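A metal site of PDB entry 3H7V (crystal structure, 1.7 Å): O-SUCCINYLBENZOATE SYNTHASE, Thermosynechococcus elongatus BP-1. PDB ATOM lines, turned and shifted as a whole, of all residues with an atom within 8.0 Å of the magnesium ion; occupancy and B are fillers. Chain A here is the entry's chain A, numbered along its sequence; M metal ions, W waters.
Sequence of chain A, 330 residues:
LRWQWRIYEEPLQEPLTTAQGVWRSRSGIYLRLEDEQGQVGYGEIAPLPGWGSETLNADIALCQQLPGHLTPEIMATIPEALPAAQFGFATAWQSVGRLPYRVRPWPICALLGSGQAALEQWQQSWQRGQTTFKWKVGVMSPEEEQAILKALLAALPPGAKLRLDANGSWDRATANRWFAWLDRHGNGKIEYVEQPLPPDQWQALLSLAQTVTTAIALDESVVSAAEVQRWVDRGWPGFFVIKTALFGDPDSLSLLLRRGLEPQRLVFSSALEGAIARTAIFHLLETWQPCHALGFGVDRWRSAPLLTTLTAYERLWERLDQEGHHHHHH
The backbone NH (N) of Glu 194 is in hydrogen-bond range of the backbone carbonyl oxygen (O) of Leu 164 (2.6 Å). The side-chain carboxylate of Glu 194 sits at hydrogen-bond distance from the side-chain hydroxyl of Tyr 192 (3.2 Å). The side-chain amino group (NZ) of Lys 134 lies close to the side-chain carboxylate (OD2) of Asp 165, at 2.9 Å. The backbone carbonyl oxygen (O) of Glu 194 is in hydrogen-bond range of the backbone NH (N) of Ala 166, at 3.1 Å. The side-chain carboxylate (OD1) of Asp 219 lies within salt-bridge range of the side-chain amino group (NZ) of Lys 243 (2.7 Å). The backbone NH (N) of Asp 219 sits at hydrogen-bond distance from the side-chain amide oxygen (OE1) of Gln 195, 2.9 Å away. N of Asn 167 lies within hydrogen-bond range of OD1 of Asp 165 (2.9 Å).
Within 4 Å of the magnesium ion: Asp 165, Glu 194 and Asp 219.
OE2 of Glu 194 binds the magnesium ion (1.9 Å). OD2 of Asp 219 binds the magnesium ion, at 2.0 Å. Water W3 binds the magnesium ion. The magnesium ion is bound by water W2 (2.1 Å). Water W1 is bound to the magnesium ion, at 2.2 Å. The magnesium ion is bound by OD2 of Asp 165, 2.2 Å away. The magnesium ion has six donor atoms within binding distance.
Water W3 lies within hydrogen-bond range of OD1 of Asp 165 (2.6 Å) and OE1 of Glu 220 (2.7 Å). Water W2 bridges the side-chain amide nitrogen of Asn 167 (2.8 Å) and the side-chain carboxylate of Glu 220 (2.9 Å).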
ATOM      1  N   TRP A  51     -13.382   4.039  -1.787  1.00  0.00           N
ATOM      2  CA  TRP A  51     -12.355   5.049  -1.570  1.00  0.00           C
ATOM      3  C   TRP A  51     -12.667   5.859  -0.311  1.00  0.00           C
ATOM      4  O   TRP A  51     -13.537   6.728  -0.312  1.00  0.00           O
ATOM      5  CB  TRP A  51     -12.255   5.962  -2.793  1.00  0.00           C
ATOM      6  CG  TRP A  51     -11.801   5.234  -4.032  1.00  0.00           C
ATOM      7  CD1 TRP A  51     -12.470   4.255  -4.702  1.00  0.00           C
ATOM      8  CD2 TRP A  51     -10.559   5.414  -4.723  1.00  0.00           C
ATOM      9  NE1 TRP A  51     -11.726   3.806  -5.766  1.00  0.00           N
ATOM     10  CE2 TRP A  51     -10.545   4.507  -5.806  1.00  0.00           C
ATOM     11  CE3 TRP A  51      -9.452   6.260  -4.529  1.00  0.00           C
ATOM     12  CZ2 TRP A  51      -9.469   4.410  -6.696  1.00  0.00           C
ATOM     13  CZ3 TRP A  51      -8.377   6.162  -5.420  1.00  0.00           C
ATOM     14  CH2 TRP A  51      -8.400   5.246  -6.480  1.00  0.00           C
ATOM     15  N   LEU A 111      -5.685   7.350 -21.353  1.00  0.00           N
ATOM     16  CA  LEU A 111      -5.472   6.024 -20.772  1.00  0.00           C
ATOM     17  C   LEU A 111      -5.139   4.974 -21.830  1.00  0.00           C
ATOM     18  O   LEU A 111      -5.624   5.036 -22.969  1.00  0.00           O
ATOM     19  CB  LEU A 111      -6.714   5.587 -19.993  1.00  0.00           C
ATOM     20  CG  LEU A 111      -7.148   6.511 -18.852  1.00  0.00           C
ATOM     21  CD1 LEU A 111      -8.405   5.949 -18.191  1.00  0.00           C
ATOM     22  CD2 LEU A 111      -6.025   6.648 -17.834  1.00  0.00           C
ATOM     23  N   LYS A 134      -1.344   7.068 -19.443  1.00  0.00           N
ATOM     24  CA  LYS A 134      -1.241   6.257 -18.240  1.00  0.00           C
ATOM     25  C   LYS A 134      -1.632   4.848 -18.641  1.00  0.00           C
ATOM     26  O   LYS A 134      -2.733   4.595 -19.111  1.00  0.00           O
ATOM     27  CB  LYS A 134      -2.162   6.758 -17.110  1.00  0.00           C
ATOM     28  CG  LYS A 134      -1.942   5.961 -15.800  1.00  0.00           C
ATOM     29  CD  LYS A 134      -2.454   6.696 -14.565  1.00  0.00           C
ATOM     30  CE  LYS A 134      -3.972   6.734 -14.497  1.00  0.00           C
ATOM     31  NZ  LYS A 134      -4.572   5.385 -14.280  1.00  0.00           N
ATOM     32  N   LEU A 164       2.645   4.907 -15.248  1.00  0.00           N
ATOM     33  CA  LEU A 164       2.324   3.491 -15.128  1.00  0.00           C
ATOM     34  C   LEU A 164       1.468   3.364 -13.884  1.00  0.00           C
ATOM     35  O   LEU A 164       1.833   3.878 -12.830  1.00  0.00           O
ATOM     36  CB  LEU A 164       3.589   2.650 -14.971  1.00  0.00           C
ATOM     37  CG  LEU A 164       4.655   2.777 -16.065  1.00  0.00           C
ATOM     38  CD1 LEU A 164       5.801   1.817 -15.758  1.00  0.00           C
ATOM     39  CD2 LEU A 164       4.060   2.454 -17.424  1.00  0.00           C
ATOM     40  N   ASP A 165       0.326   2.704 -13.991  1.00  0.00           N
ATOM     41  CA  ASP A 165      -0.533   2.554 -12.822  1.00  0.00           C
ATOM     42  C   ASP A 165      -0.673   1.089 -12.444  1.00  0.00           C
ATOM     43  O   ASP A 165      -1.268   0.300 -13.171  1.00  0.00           O
ATOM     44  CB  ASP A 165      -1.917   3.157 -13.085  1.00  0.00           C
ATOM     45  CG  ASP A 165      -2.678   3.422 -11.799  1.00  0.00           C
ATOM     46  OD1 ASP A 165      -2.404   2.742 -10.789  1.00  0.00           O
ATOM     47  OD2 ASP A 165      -3.572   4.298 -11.800  1.00  0.00           O
ATOM     48  N   ALA A 166      -0.111   0.719 -11.286  1.00  0.00           N
ATOM     49  CA  ALA A 166      -0.186  -0.650 -10.824  1.00  0.00           C
ATOM     50  C   ALA A 166      -1.421  -0.918  -9.967  1.00  0.00           C
ATOM     51  O   ALA A 166      -1.697  -2.060  -9.601  1.00  0.00           O
ATOM     52  CB  ALA A 166       1.068  -1.004 -10.037  1.00  0.00           C
ATOM     53  N   ASN A 167      -2.167   0.140  -9.645  1.00  0.00           N
ATOM     54  CA  ASN A 167      -3.376   0.021  -8.833  1.00  0.00           C
ATOM     55  C   ASN A 167      -3.138  -0.757  -7.537  1.00  0.00           C
ATOM     56  O   ASN A 167      -4.025  -1.463  -7.056  1.00  0.00           O
ATOM     57  CB  ASN A 167      -4.505  -0.642  -9.635  1.00  0.00           C
ATOM     58  CG  ASN A 167      -4.877   0.148 -10.881  1.00  0.00           C
ATOM     59  OD1 ASN A 167      -4.500  -0.204 -11.990  1.00  0.00           O
ATOM     60  ND2 ASN A 167      -5.615   1.231 -10.685  1.00  0.00           N
ATOM     61  N   GLY A 168      -1.940  -0.604  -6.985  1.00  0.00           N
ATOM     62  CA  GLY A 168      -1.563  -1.281  -5.754  1.00  0.00           C
ATOM     63  C   GLY A 168      -1.582  -2.786  -5.833  1.00  0.00           C
ATOM     64  O   GLY A 168      -1.767  -3.467  -4.820  1.00  0.00           O
ATOM     65  N   TYR A 192       5.972   8.830 -13.775  1.00  0.00           N
ATOM     66  CA  TYR A 192       5.922   8.196 -12.462  1.00  0.00           C
ATOM     67  C   TYR A 192       5.186   6.876 -12.489  1.00  0.00           C
ATOM     68  O   TYR A 192       4.540   6.528 -13.488  1.00  0.00           O
ATOM     69  CB  TYR A 192       5.256   9.115 -11.422  1.00  0.00           C
ATOM     70  CG  TYR A 192       3.811   9.529 -11.694  1.00  0.00           C
ATOM     71  CD1 TYR A 192       3.489  10.864 -11.925  1.00  0.00           C
ATOM     72  CD2 TYR A 192       2.766   8.596 -11.648  1.00  0.00           C
ATOM     73  CE1 TYR A 192       2.161  11.269 -12.097  1.00  0.00           C
ATOM     74  CE2 TYR A 192       1.438   9.001 -11.821  1.00  0.00           C
ATOM     75  CZ  TYR A 192       1.144  10.330 -12.043  1.00  0.00           C
ATOM     76  OH  TYR A 192      -0.169  10.726 -12.187  1.00  0.00           O
ATOM     77  N   GLU A 194       2.289   4.972 -10.558  1.00  0.00           N
ATOM     78  CA  GLU A 194       1.181   5.261  -9.653  1.00  0.00           C
ATOM     79  C   GLU A 194       0.821   4.060  -8.785  1.00  0.00           C
ATOM     80  O   GLU A 194       0.600   2.967  -9.288  1.00  0.00           O
ATOM     81  CB  GLU A 194      -0.042   5.711 -10.466  1.00  0.00           C
ATOM     82  CG  GLU A 194      -1.095   6.506  -9.695  1.00  0.00           C
ATOM     83  CD  GLU A 194      -2.112   7.184 -10.612  1.00  0.00           C
ATOM     84  OE1 GLU A 194      -1.736   8.127 -11.332  1.00  0.00           O
ATOM     85  OE2 GLU A 194      -3.280   6.763 -10.613  1.00  0.00           O
ATOM     86  N   GLN A 195       0.789   4.286  -7.472  1.00  0.00           N
ATOM     87  CA  GLN A 195       0.436   3.265  -6.469  1.00  0.00           C
ATOM     88  C   GLN A 195       1.034   1.881  -6.734  1.00  0.00           C
ATOM     89  O   GLN A 195       0.315   0.921  -7.007  1.00  0.00           O
ATOM     90  CB  GLN A 195      -1.095   3.171  -6.378  1.00  0.00           C
ATOM     91  CG  GLN A 195      -1.627   2.584  -5.072  1.00  0.00           C
ATOM     92  CD  GLN A 195      -1.473   3.538  -3.896  1.00  0.00           C
ATOM     93  OE1 GLN A 195      -1.796   4.721  -3.989  1.00  0.00           O
ATOM     94  NE2 GLN A 195      -0.986   3.011  -2.768  1.00  0.00           N
ATOM     95  N   ALA A 217       3.762   7.942  -7.388  1.00  0.00           N
ATOM     96  CA  ALA A 217       2.581   8.739  -7.094  1.00  0.00           C
ATOM     97  C   ALA A 217       1.594   7.964  -6.227  1.00  0.00           C
ATOM     98  O   ALA A 217       1.371   6.773  -6.441  1.00  0.00           O
ATOM     99  CB  ALA A 217       1.893   9.184  -8.383  1.00  0.00           C
ATOM    100  N   LEU A 218       0.997   8.658  -5.262  1.00  0.00           N
ATOM    101  CA  LEU A 218      -0.003   8.041  -4.396  1.00  0.00           C
ATOM    102  C   LEU A 218      -1.365   8.365  -4.988  1.00  0.00           C
ATOM    103  O   LEU A 218      -1.631   9.499  -5.384  1.00  0.00           O
ATOM    104  CB  LEU A 218       0.084   8.611  -2.987  1.00  0.00           C
ATOM    105  CG  LEU A 218       1.390   8.325  -2.254  1.00  0.00           C
ATOM    106  CD1 LEU A 218       1.392   9.071  -0.938  1.00  0.00           C
ATOM    107  CD2 LEU A 218       1.558   6.830  -2.033  1.00  0.00           C
ATOM    108  N   ASP A 219      -2.241   7.358  -5.046  1.00  0.00           N
ATOM    109  CA  ASP A 219      -3.583   7.555  -5.588  1.00  0.00           C
ATOM    110  C   ASP A 219      -4.557   6.952  -4.588  1.00  0.00           C
ATOM    111  O   ASP A 219      -5.187   7.665  -3.807  1.00  0.00           O
ATOM    112  CB  ASP A 219      -3.702   6.885  -6.959  1.00  0.00           C
ATOM    113  CG  ASP A 219      -5.075   7.083  -7.601  1.00  0.00           C
ATOM    114  OD1 ASP A 219      -5.908   7.828  -7.025  1.00  0.00           O
ATOM    115  OD2 ASP A 219      -5.327   6.493  -8.667  1.00  0.00           O
ATOM    116  N   GLU A 220      -4.646   5.618  -4.581  1.00  0.00           N
ATOM    117  CA  GLU A 220      -5.525   4.927  -3.652  1.00  0.00           C
ATOM    118  C   GLU A 220      -5.196   5.301  -2.200  1.00  0.00           C
ATOM    119  O   GLU A 220      -6.070   5.305  -1.334  1.00  0.00           O
ATOM    120  CB  GLU A 220      -5.387   3.405  -3.840  1.00  0.00           C
ATOM    121  CG  GLU A 220      -6.153   2.842  -5.042  1.00  0.00           C
ATOM    122  CD  GLU A 220      -5.404   2.968  -6.365  1.00  0.00           C
ATOM    123  OE1 GLU A 220      -4.354   3.623  -6.426  1.00  0.00           O
ATOM    124  OE2 GLU A 220      -5.903   2.387  -7.365  1.00  0.00           O
ATOM    125  N   VAL A 241      -1.958  12.208  -6.195  1.00  0.00           N
ATOM    126  CA  VAL A 241      -3.042  12.275  -7.172  1.00  0.00           C
ATOM    127  C   VAL A 241      -4.251  12.758  -6.378  1.00  0.00           C
ATOM    128  O   VAL A 241      -4.800  12.038  -5.536  1.00  0.00           O
ATOM    129  CB  VAL A 241      -3.316  10.896  -7.797  1.00  0.00           C
ATOM    130  CG1 VAL A 241      -4.560  10.960  -8.694  1.00  0.00           C
ATOM    131  CG2 VAL A 241      -2.099  10.451  -8.615  1.00  0.00           C
ATOM    132  N   LYS A 243      -8.072  13.826  -5.931  1.00  0.00           N
ATOM    133  CA  LYS A 243      -9.416  13.697  -6.476  1.00  0.00           C
ATOM    134  C   LYS A 243     -10.175  14.768  -5.717  1.00  0.00           C
ATOM    135  O   LYS A 243     -10.710  14.519  -4.629  1.00  0.00           O
ATOM    136  CB  LYS A 243     -10.007  12.322  -6.176  1.00  0.00           C
ATOM    137  CG  LYS A 243      -9.530  11.215  -7.118  1.00  0.00           C
ATOM    138  CD  LYS A 243      -8.065  10.824  -6.874  1.00  0.00           C
ATOM    139  CE  LYS A 243      -7.880  10.226  -5.480  1.00  0.00           C
ATOM    140  NZ  LYS A 243      -6.461   9.827  -5.243  1.00  0.00           N
ATOM    141  N   SER A 269      -7.034  14.498 -10.620  1.00  0.00           N
ATOM    142  CA  SER A 269      -7.725  13.450 -11.346  1.00  0.00           C
ATOM    143  C   SER A 269      -9.203  13.292 -11.039  1.00  0.00           C
ATOM    144  O   SER A 269      -9.718  13.842 -10.067  1.00  0.00           O
ATOM    145  CB  SER A 269      -7.002  12.123 -11.122  1.00  0.00           C
ATOM    146  OG  SER A 269      -5.664  12.215 -11.616  1.00  0.00           O
HETATM  147 MG    MG M   1      -4.516   5.356 -10.153  1.00  0.00          MG
HETATM  148  O   HOH W   1      -5.933   6.093 -11.602  1.00  0.00           O
HETATM  149  O   HOH W   2      -5.984   3.893  -9.796  1.00  0.00           O
HETATM  150  O   HOH W   3      -3.309   4.256  -8.860  1.00  0.00           O
